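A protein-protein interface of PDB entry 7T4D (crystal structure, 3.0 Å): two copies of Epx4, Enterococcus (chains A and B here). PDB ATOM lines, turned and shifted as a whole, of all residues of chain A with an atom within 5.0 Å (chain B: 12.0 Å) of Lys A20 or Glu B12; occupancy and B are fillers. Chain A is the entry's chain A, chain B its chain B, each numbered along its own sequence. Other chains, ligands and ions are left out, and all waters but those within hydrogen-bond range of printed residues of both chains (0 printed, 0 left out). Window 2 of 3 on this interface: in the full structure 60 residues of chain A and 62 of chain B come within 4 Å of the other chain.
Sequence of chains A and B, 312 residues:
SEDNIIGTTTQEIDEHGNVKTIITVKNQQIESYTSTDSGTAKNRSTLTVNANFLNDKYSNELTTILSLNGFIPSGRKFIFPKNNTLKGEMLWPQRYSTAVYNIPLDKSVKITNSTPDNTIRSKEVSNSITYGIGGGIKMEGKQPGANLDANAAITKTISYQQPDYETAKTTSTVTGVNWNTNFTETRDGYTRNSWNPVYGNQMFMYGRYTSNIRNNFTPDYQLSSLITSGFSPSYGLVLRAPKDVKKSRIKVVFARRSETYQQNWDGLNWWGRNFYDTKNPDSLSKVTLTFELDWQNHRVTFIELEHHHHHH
Lys A20 touches Glu B12, but with the chains exchanged Glu A12 does not touch Lys B20 (11.3 Å). Thr A21 touches Gln B11, but with the chains exchanged Gln A11 does not touch Thr B21 (15.5 Å). Thr A21 touches Glu B12, but with the chains exchanged Glu A12 does not touch Thr B21 (14.0 Å). Ile A22 touches Gln B11, but with the chains exchanged Gln A11 does not touch Ile B22 (13.9 Å). Of the 9 pairs that touch across the chains among the printed residues, none has its exchanged pair printed and touching as well.
Of the 8 printed residues of chain A, 4 touch a printed residue of chain B. Printed residues of chain A that touch a printed residue of chain B: Val A19, Lys A20, Thr A21 and Ile A22. Hydrophobic or aromatic side chains of chain A that line the printed part of chain B: Ile A22. Hydrophobic or aromatic side chains of chain B that line the printed part of chain A: Ile B13. Among the printed residues, 9 pairs touch across the chains. Among the printed residues, Asp or Glu carboxylates within 4 Å of a Lys or Arg side-chain nitrogen of the other chain: Lys A20 with Glu B12 (3.1 Å).
OE1 of Glu B12 lies within salt-bridge range of NZ of Lys A20 (3.1 Å). The backbone NH (N) of Glu B15 lies within hydrogen-bond range of the backbone carbonyl oxygen (O) of Val A19 (3.5 Å). N of Ile B13 lies within hydrogen-bond range of O of Thr A21.
The side-chain amide nitrogen of Gln A11 is in hydrogen-bond range of the side-chain hydroxyl of Thr A21 (3.1 Å). OD1 of Asp B14 is in hydrogen-bond range of N of Gly B17, 3.1 Å away. The backbone NH of Asn B18 lies within hydrogen-bond range of the side-chain carboxylate of Asp B14 (2.8 Å). O of Lys B20 lies within hydrogen-bond range of N of Glu B12, 2.8 Å away. N of Thr A10 sits at hydrogen-bond distance from O of Ile A22, at 2.9 Å. NE2 of Gln B11 lies within hydrogen-bond range of OG1 of Thr B21, 3.2 Å away.
No residue of chain B comes within 4 Å of Gln A11. No residue of chain B comes within 4 Å of Glu A12. Of chain B, only Asp B14 (3.8 Å) and Glu B15 (3.5 Å) come within 4 Å of Val A19. Printed residues of chain B within 4 Å of Lys A20: Glu B12 (3.1 Å) and Ile B13 (3.5 Å). Of chain B, only Thr B10 and Gln B11 come within 4 Å of Ile A22. Of the printed residues of chain A, Thr B10 touches Ile A22 (3.5 Å). Glu B12 touches just these residues of chain A: Lys A20 and Thr A21. Printed residues of chain A within 4 Å of Asp B14: Val A19. Printed residues of chain A within 4 Å of Glu B15: Val A19. Val B19 touches none of the printed residues of chain A. The nearest residue of chain B that does not touch Lys A20 is Asp B14 (4.5 Å).
Among the printed residues, merely in contact across the chains: Thr A21 with Glu B12 (3.4 Å), Ile A22 with Gln B11 (3.5 Å), Lys A20 with Ile B13 (3.5 Å), Ile A22 with Thr B10 (3.5 Å), Thr A21 with Gln B11 (3.6 Å) and Val A19 with Asp B14 (3.8 Å).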
ATOM      1  N   THR A  10      -5.771 -11.345 -31.412  1.00  0.00           N
ATOM      2  CA  THR A  10      -4.524 -11.220 -32.157  1.00  0.00           C
ATOM      3  C   THR A  10      -3.869 -12.577 -32.361  1.00  0.00           C
ATOM      4  O   THR A  10      -3.917 -13.440 -31.486  1.00  0.00           O
ATOM      5  CB  THR A  10      -3.527 -10.288 -31.443  1.00  0.00           C
ATOM      6  OG1 THR A  10      -4.192  -9.082 -31.047  1.00  0.00           O
ATOM      7  CG2 THR A  10      -2.368  -9.942 -32.366  1.00  0.00           C
ATOM      8  N   GLN A  11      -3.257 -12.759 -33.525  1.00  0.00           N
ATOM      9  CA  GLN A  11      -2.516 -13.977 -33.818  1.00  0.00           C
ATOM     10  C   GLN A  11      -1.154 -13.656 -34.418  1.00  0.00           C
ATOM     11  O   GLN A  11      -1.060 -12.961 -35.430  1.00  0.00           O
ATOM     12  CB  GLN A  11      -3.310 -14.875 -34.769  1.00  0.00           C
ATOM     13  CG  GLN A  11      -4.601 -15.420 -34.180  1.00  0.00           C
ATOM     14  CD  GLN A  11      -4.943 -16.799 -34.711  1.00  0.00           C
ATOM     15  OE1 GLN A  11      -4.754 -17.086 -35.893  1.00  0.00           O
ATOM     16  NE2 GLN A  11      -5.454 -17.660 -33.837  1.00  0.00           N
ATOM     17  N   GLU A  12      -0.100 -14.160 -33.786  1.00  0.00           N
ATOM     18  CA  GLU A  12       1.247 -13.991 -34.308  1.00  0.00           C
ATOM     19  C   GLU A  12       1.695 -15.298 -34.946  1.00  0.00           C
ATOM     20  O   GLU A  12       1.599 -16.363 -34.337  1.00  0.00           O
ATOM     21  CB  GLU A  12       2.220 -13.556 -33.209  1.00  0.00           C
ATOM     22  CG  GLU A  12       1.668 -12.492 -32.274  1.00  0.00           C
ATOM     23  CD  GLU A  12       2.749 -11.835 -31.433  1.00  0.00           C
ATOM     24  OE1 GLU A  12       3.832 -12.439 -31.275  1.00  0.00           O
ATOM     25  OE2 GLU A  12       2.517 -10.711 -30.935  1.00  0.00           O
ATOM     26  N   ASN A  18       4.725 -21.375 -36.164  1.00  0.00           N
ATOM     27  CA  ASN A  18       4.297 -21.310 -34.775  1.00  0.00           C
ATOM     28  C   ASN A  18       3.227 -20.238 -34.628  1.00  0.00           C
ATOM     29  O   ASN A  18       3.324 -19.172 -35.234  1.00  0.00           O
ATOM     30  CB  ASN A  18       5.479 -21.018 -33.848  1.00  0.00           C
ATOM     31  CG  ASN A  18       6.513 -22.127 -33.852  1.00  0.00           C
ATOM     32  OD1 ASN A  18       6.177 -23.303 -33.980  1.00  0.00           O
ATOM     33  ND2 ASN A  18       7.778 -21.756 -33.706  1.00  0.00           N
ATOM     34  N   VAL A  19       2.206 -20.519 -33.827  1.00  0.00           N
ATOM     35  CA  VAL A  19       1.101 -19.583 -33.686  1.00  0.00           C
ATOM     36  C   VAL A  19       0.837 -19.211 -32.236  1.00  0.00           C
ATOM     37  O   VAL A  19       0.618 -20.074 -31.387  1.00  0.00           O
ATOM     38  CB  VAL A  19      -0.193 -20.154 -34.291  1.00  0.00           C
ATOM     39  CG1 VAL A  19      -1.336 -19.161 -34.133  1.00  0.00           C
ATOM     40  CG2 VAL A  19       0.020 -20.505 -35.755  1.00  0.00           C
ATOM     41  N   LYS A  20       0.851 -17.911 -31.967  1.00  0.00           N
ATOM     42  CA  LYS A  20       0.518 -17.390 -30.652  1.00  0.00           C
ATOM     43  C   LYS A  20      -0.803 -16.642 -30.743  1.00  0.00           C
ATOM     44  O   LYS A  20      -1.057 -15.936 -31.721  1.00  0.00           O
ATOM     45  CB  LYS A  20       1.624 -16.472 -30.134  1.00  0.00           C
ATOM     46  CG  LYS A  20       1.312 -15.808 -28.802  1.00  0.00           C
ATOM     47  CD  LYS A  20       2.502 -15.011 -28.293  1.00  0.00           C
ATOM     48  CE  LYS A  20       2.303 -14.573 -26.852  1.00  0.00           C
ATOM     49  NZ  LYS A  20       3.338 -13.588 -26.427  1.00  0.00           N
ATOM     50  N   THR A  21      -1.647 -16.797 -29.731  1.00  0.00           N
ATOM     51  CA  THR A  21      -2.944 -16.135 -29.732  1.00  0.00           C
ATOM     52  C   THR A  21      -3.114 -15.277 -28.487  1.00  0.00           C
ATOM     53  O   THR A  21      -2.899 -15.736 -27.367  1.00  0.00           O
ATOM     54  CB  THR A  21      -4.103 -17.147 -29.818  1.00  0.00           C
ATOM     55  OG1 THR A  21      -4.073 -17.807 -31.090  1.00  0.00           O
ATOM     56  CG2 THR A  21      -5.437 -16.437 -29.658  1.00  0.00           C
ATOM     57  N   ILE A  22      -3.501 -14.025 -28.695  1.00  0.00           N
ATOM     58  CA  ILE A  22      -3.694 -13.094 -27.596  1.00  0.00           C
ATOM     59  C   ILE A  22      -5.109 -12.544 -27.637  1.00  0.00           C
ATOM     60  O   ILE A  22      -5.512 -11.917 -28.616  1.00  0.00           O
ATOM     61  CB  ILE A  22      -2.687 -11.932 -27.649  1.00  0.00           C
ATOM     62  CG1 ILE A  22      -1.260 -12.470 -27.785  1.00  0.00           C
ATOM     63  CG2 ILE A  22      -2.816 -11.063 -26.411  1.00  0.00           C
ATOM     64  CD1 ILE A  22      -0.197 -11.392 -27.779  1.00  0.00           C
ATOM     65  N   THR B   8      -8.723  -3.972 -18.269  1.00  0.00           N
ATOM     66  CA  THR B   8      -8.682  -4.971 -19.326  1.00  0.00           C
ATOM     67  C   THR B   8      -8.138  -6.308 -18.827  1.00  0.00           C
ATOM     68  O   THR B   8      -7.271  -6.355 -17.955  1.00  0.00           O
ATOM     69  CB  THR B   8      -7.819  -4.496 -20.506  1.00  0.00           C
ATOM     70  OG1 THR B   8      -8.036  -5.349 -21.634  1.00  0.00           O
ATOM     71  CG2 THR B   8      -6.342  -4.516 -20.133  1.00  0.00           C
ATOM     72  N   THR B   9      -8.656  -7.395 -19.392  1.00  0.00           N
ATOM     73  CA  THR B   9      -8.170  -8.732 -19.077  1.00  0.00           C
ATOM     74  C   THR B   9      -7.640  -9.395 -20.341  1.00  0.00           C
ATOM     75  O   THR B   9      -8.317  -9.420 -21.368  1.00  0.00           O
ATOM     76  CB  THR B   9      -9.271  -9.611 -18.460  1.00  0.00           C
ATOM     77  OG1 THR B   9      -9.748  -9.004 -17.253  1.00  0.00           O
ATOM     78  CG2 THR B   9      -8.731 -10.998 -18.143  1.00  0.00           C
ATOM     79  N   THR B  10      -6.427  -9.931 -20.261  1.00  0.00           N
ATOM     80  CA  THR B  10      -5.774 -10.513 -21.425  1.00  0.00           C
ATOM     81  C   THR B  10      -5.270 -11.926 -21.154  1.00  0.00           C
ATOM     82  O   THR B  10      -4.820 -12.231 -20.051  1.00  0.00           O
ATOM     83  CB  THR B  10      -4.590  -9.647 -21.889  1.00  0.00           C
ATOM     84  OG1 THR B  10      -4.996  -8.274 -21.951  1.00  0.00           O
ATOM     85  CG2 THR B  10      -4.107 -10.093 -23.260  1.00  0.00           C
ATOM     86  N   GLN B  11      -5.352 -12.783 -22.167  1.00  0.00           N
ATOM     87  CA  GLN B  11      -4.806 -14.133 -22.080  1.00  0.00           C
ATOM     88  C   GLN B  11      -3.975 -14.454 -23.317  1.00  0.00           C
ATOM     89  O   GLN B  11      -4.465 -14.373 -24.443  1.00  0.00           O
ATOM     90  CB  GLN B  11      -5.923 -15.166 -21.916  1.00  0.00           C
ATOM     91  CG  GLN B  11      -6.689 -15.059 -20.610  1.00  0.00           C
ATOM     92  CD  GLN B  11      -7.162 -16.409 -20.105  1.00  0.00           C
ATOM     93  OE1 GLN B  11      -7.584 -17.263 -20.884  1.00  0.00           O
ATOM     94  NE2 GLN B  11      -7.095 -16.607 -18.793  1.00  0.00           N
ATOM     95  N   GLU B  12      -2.716 -14.815 -23.099  1.00  0.00           N
ATOM     96  CA  GLU B  12      -1.832 -15.193 -24.192  1.00  0.00           C
ATOM     97  C   GLU B  12      -1.624 -16.703 -24.225  1.00  0.00           C
ATOM     98  O   GLU B  12      -1.258 -17.306 -23.217  1.00  0.00           O
ATOM     99  CB  GLU B  12      -0.489 -14.474 -24.050  1.00  0.00           C
ATOM    100  CG  GLU B  12      -0.621 -13.019 -23.624  1.00  0.00           C
ATOM    101  CD  GLU B  12       0.667 -12.236 -23.801  1.00  0.00           C
ATOM    102  OE1 GLU B  12       1.744 -12.867 -23.877  1.00  0.00           O
ATOM    103  OE2 GLU B  12       0.603 -10.987 -23.860  1.00  0.00           O
ATOM    104  N   ILE B  13      -1.861 -17.313 -25.383  1.00  0.00           N
ATOM    105  CA  ILE B  13      -1.684 -18.753 -25.528  1.00  0.00           C
ATOM    106  C   ILE B  13      -0.632 -19.092 -26.583  1.00  0.00           C
ATOM    107  O   ILE B  13      -0.860 -18.891 -27.776  1.00  0.00           O
ATOM    108  CB  ILE B  13      -3.008 -19.441 -25.908  1.00  0.00           C
ATOM    109  CG1 ILE B  13      -4.065 -19.212 -24.822  1.00  0.00           C
ATOM    110  CG2 ILE B  13      -2.787 -20.926 -26.160  1.00  0.00           C
ATOM    111  CD1 ILE B  13      -5.183 -18.279 -25.244  1.00  0.00           C
ATOM    112  N   ASP B  14       0.514 -19.609 -26.147  1.00  0.00           N
ATOM    113  CA  ASP B  14       1.594 -19.955 -27.071  1.00  0.00           C
ATOM    114  C   ASP B  14       1.266 -21.217 -27.871  1.00  0.00           C
ATOM    115  O   ASP B  14       0.185 -21.792 -27.735  1.00  0.00           O
ATOM    116  CB  ASP B  14       2.939 -20.102 -26.345  1.00  0.00           C
ATOM    117  CG  ASP B  14       2.919 -21.145 -25.246  1.00  0.00           C
ATOM    118  OD1 ASP B  14       2.096 -22.083 -25.296  1.00  0.00           O
ATOM    119  OD2 ASP B  14       3.757 -21.027 -24.328  1.00  0.00           O
ATOM    120  N   GLU B  15       2.214 -21.641 -28.699  1.00  0.00           N
ATOM    121  CA  GLU B  15       2.036 -22.792 -29.580  1.00  0.00           C
ATOM    122  C   GLU B  15       2.008 -24.139 -28.856  1.00  0.00           C
ATOM    123  O   GLU B  15       1.858 -25.182 -29.493  1.00  0.00           O
ATOM    124  CB  GLU B  15       3.161 -22.821 -30.618  1.00  0.00           C
ATOM    125  CG  GLU B  15       4.569 -22.833 -30.016  1.00  0.00           C
ATOM    126  CD  GLU B  15       5.021 -21.473 -29.508  1.00  0.00           C
ATOM    127  OE1 GLU B  15       4.168 -20.574 -29.358  1.00  0.00           O
ATOM    128  OE2 GLU B  15       6.234 -21.308 -29.253  1.00  0.00           O
ATOM    129  N   HIS B  16       2.155 -24.129 -27.534  1.00  0.00           N
ATOM    130  CA  HIS B  16       2.164 -25.379 -26.774  1.00  0.00           C
ATOM    131  C   HIS B  16       1.068 -25.463 -25.713  1.00  0.00           C
ATOM    132  O   HIS B  16       1.056 -26.385 -24.897  1.00  0.00           O
ATOM    133  CB  HIS B  16       3.535 -25.583 -26.126  1.00  0.00           C
ATOM    134  CG  HIS B  16       4.637 -25.793 -27.117  1.00  0.00           C
ATOM    135  ND1 HIS B  16       5.914 -25.311 -26.924  1.00  0.00           N
ATOM    136  CD2 HIS B  16       4.653 -26.434 -28.309  1.00  0.00           C
ATOM    137  CE1 HIS B  16       6.669 -25.646 -27.957  1.00  0.00           C
ATOM    138  NE2 HIS B  16       5.927 -26.328 -28.810  1.00  0.00           N
ATOM    139  N   GLY B  17       0.150 -24.503 -25.727  1.00  0.00           N
ATOM    140  CA  GLY B  17      -0.976 -24.512 -24.811  1.00  0.00           C
ATOM    141  C   GLY B  17      -0.704 -23.835 -23.482  1.00  0.00           C
ATOM    142  O   GLY B  17      -1.508 -23.928 -22.555  1.00  0.00           O
ATOM    143  N   ASN B  18       0.434 -23.157 -23.384  1.00  0.00           N
ATOM    144  CA  ASN B  18       0.751 -22.379 -22.193  1.00  0.00           C
ATOM    145  C   ASN B  18      -0.092 -21.110 -22.168  1.00  0.00           C
ATOM    146  O   ASN B  18      -0.317 -20.488 -23.207  1.00  0.00           O
ATOM    147  CB  ASN B  18       2.237 -22.030 -22.146  1.00  0.00           C
ATOM    148  CG  ASN B  18       3.123 -23.254 -22.027  1.00  0.00           C
ATOM    149  OD1 ASN B  18       2.762 -24.236 -21.378  1.00  0.00           O
ATOM    150  ND2 ASN B  18       4.291 -23.202 -22.658  1.00  0.00           N
ATOM    151  N   VAL B  19      -0.560 -20.725 -20.987  1.00  0.00           N
ATOM    152  CA  VAL B  19      -1.436 -19.566 -20.881  1.00  0.00           C
ATOM    153  C   VAL B  19      -0.918 -18.529 -19.892  1.00  0.00           C
ATOM    154  O   VAL B  19      -0.648 -18.838 -18.731  1.00  0.00           O
ATOM    155  CB  VAL B  19      -2.859 -19.980 -20.464  1.00  0.00           C
ATOM    156  CG1 VAL B  19      -3.762 -18.758 -20.372  1.00  0.00           C
ATOM    157  CG2 VAL B  19      -3.423 -20.991 -21.450  1.00  0.00           C
ATOM    158  N   LYS B  20      -0.784 -17.296 -20.368  1.00  0.00           N
ATOM    159  CA  LYS B  20      -0.390 -16.167 -19.534  1.00  0.00           C
ATOM    160  C   LYS B  20      -1.575 -15.222 -19.373  1.00  0.00           C
ATOM    161  O   LYS B  20      -2.335 -15.003 -20.318  1.00  0.00           O
ATOM    162  CB  LYS B  20       0.803 -15.425 -20.141  1.00  0.00           C
ATOM    163  CG  LYS B  20       1.203 -14.167 -19.378  1.00  0.00           C
ATOM    164  CD  LYS B  20       2.458 -13.530 -19.955  1.00  0.00           C
ATOM    165  CE  LYS B  20       2.996 -12.441 -19.039  1.00  0.00           C
ATOM    166  NZ  LYS B  20       4.068 -11.638 -19.690  1.00  0.00           N
ATOM    167  N   THR B  21      -1.733 -14.662 -18.179  1.00  0.00           N
ATOM    168  CA  THR B  21      -2.852 -13.767 -17.907  1.00  0.00           C
ATOM    169  C   THR B  21      -2.386 -12.396 -17.426  1.00  0.00           C
ATOM    170  O   THR B  21      -1.578 -12.290 -16.504  1.00  0.00           O
ATOM    171  CB  THR B  21      -3.802 -14.365 -16.857  1.00  0.00           C
ATOM    172  OG1 THR B  21      -4.434 -15.535 -17.392  1.00  0.00           O
ATOM    173  CG2 THR B  21      -4.868 -13.353 -16.466  1.00  0.00           C
ATOM    174  N   ILE B  22      -2.906 -11.352 -18.062  1.00  0.00           N
ATOM    175  CA  ILE B  22      -2.545  -9.981 -17.725  1.00  0.00           C
ATOM    176  C   ILE B  22      -3.790  -9.169 -17.384  1.00  0.00           C
ATOM    177  O   ILE B  22      -4.688  -9.022 -18.212  1.00  0.00           O
ATOM    178  CB  ILE B  22      -1.789  -9.299 -18.884  1.00  0.00           C
ATOM    179  CG1 ILE B  22      -0.633 -10.181 -19.360  1.00  0.00           C
ATOM    180  CG2 ILE B  22      -1.287  -7.928 -18.462  1.00  0.00           C
ATOM    181  CD1 ILE B  22       0.200  -9.559 -20.460  1.00  0.00           C
ATOM    182  N   ILE B  23      -3.840  -8.645 -16.164  1.00  0.00           N
ATOM    183  CA  ILE B  23      -4.983  -7.852 -15.720  1.00  0.00           C
ATOM    184  C   ILE B  23      -4.588  -6.419 -15.389  1.00  0.00           C
ATOM    185  O   ILE B  23      -3.664  -6.180 -14.612  1.00  0.00           O
ATOM    186  CB  ILE B  23      -5.663  -8.476 -14.493  1.00  0.00           C
ATOM    187  CG1 ILE B  23      -6.174  -9.878 -14.829  1.00  0.00           C
ATOM    188  CG2 ILE B  23      -6.822  -7.609 -14.034  1.00  0.00           C
ATOM    189  CD1 ILE B  23      -7.388 -10.291 -14.027  1.00  0.00           C
ATOM    190  N   THR B  24      -5.297  -5.468 -15.989  1.00  0.00           N
ATOM    191  CA  THR B  24      -5.023  -4.051 -15.790  1.00  0.00           C
ATOM    192  C   THR B  24      -6.255  -3.320 -15.262  1.00  0.00           C
ATOM    193  O   THR B  24      -7.338  -3.428 -15.832  1.00  0.00           O
ATOM    194  CB  THR B  24      -4.561  -3.380 -17.098  1.00  0.00           C
ATOM    195  OG1 THR B  24      -3.321  -3.959 -17.526  1.00  0.00           O
ATOM    196  CG2 THR B  24      -4.373  -1.885 -16.895  1.00  0.00           C
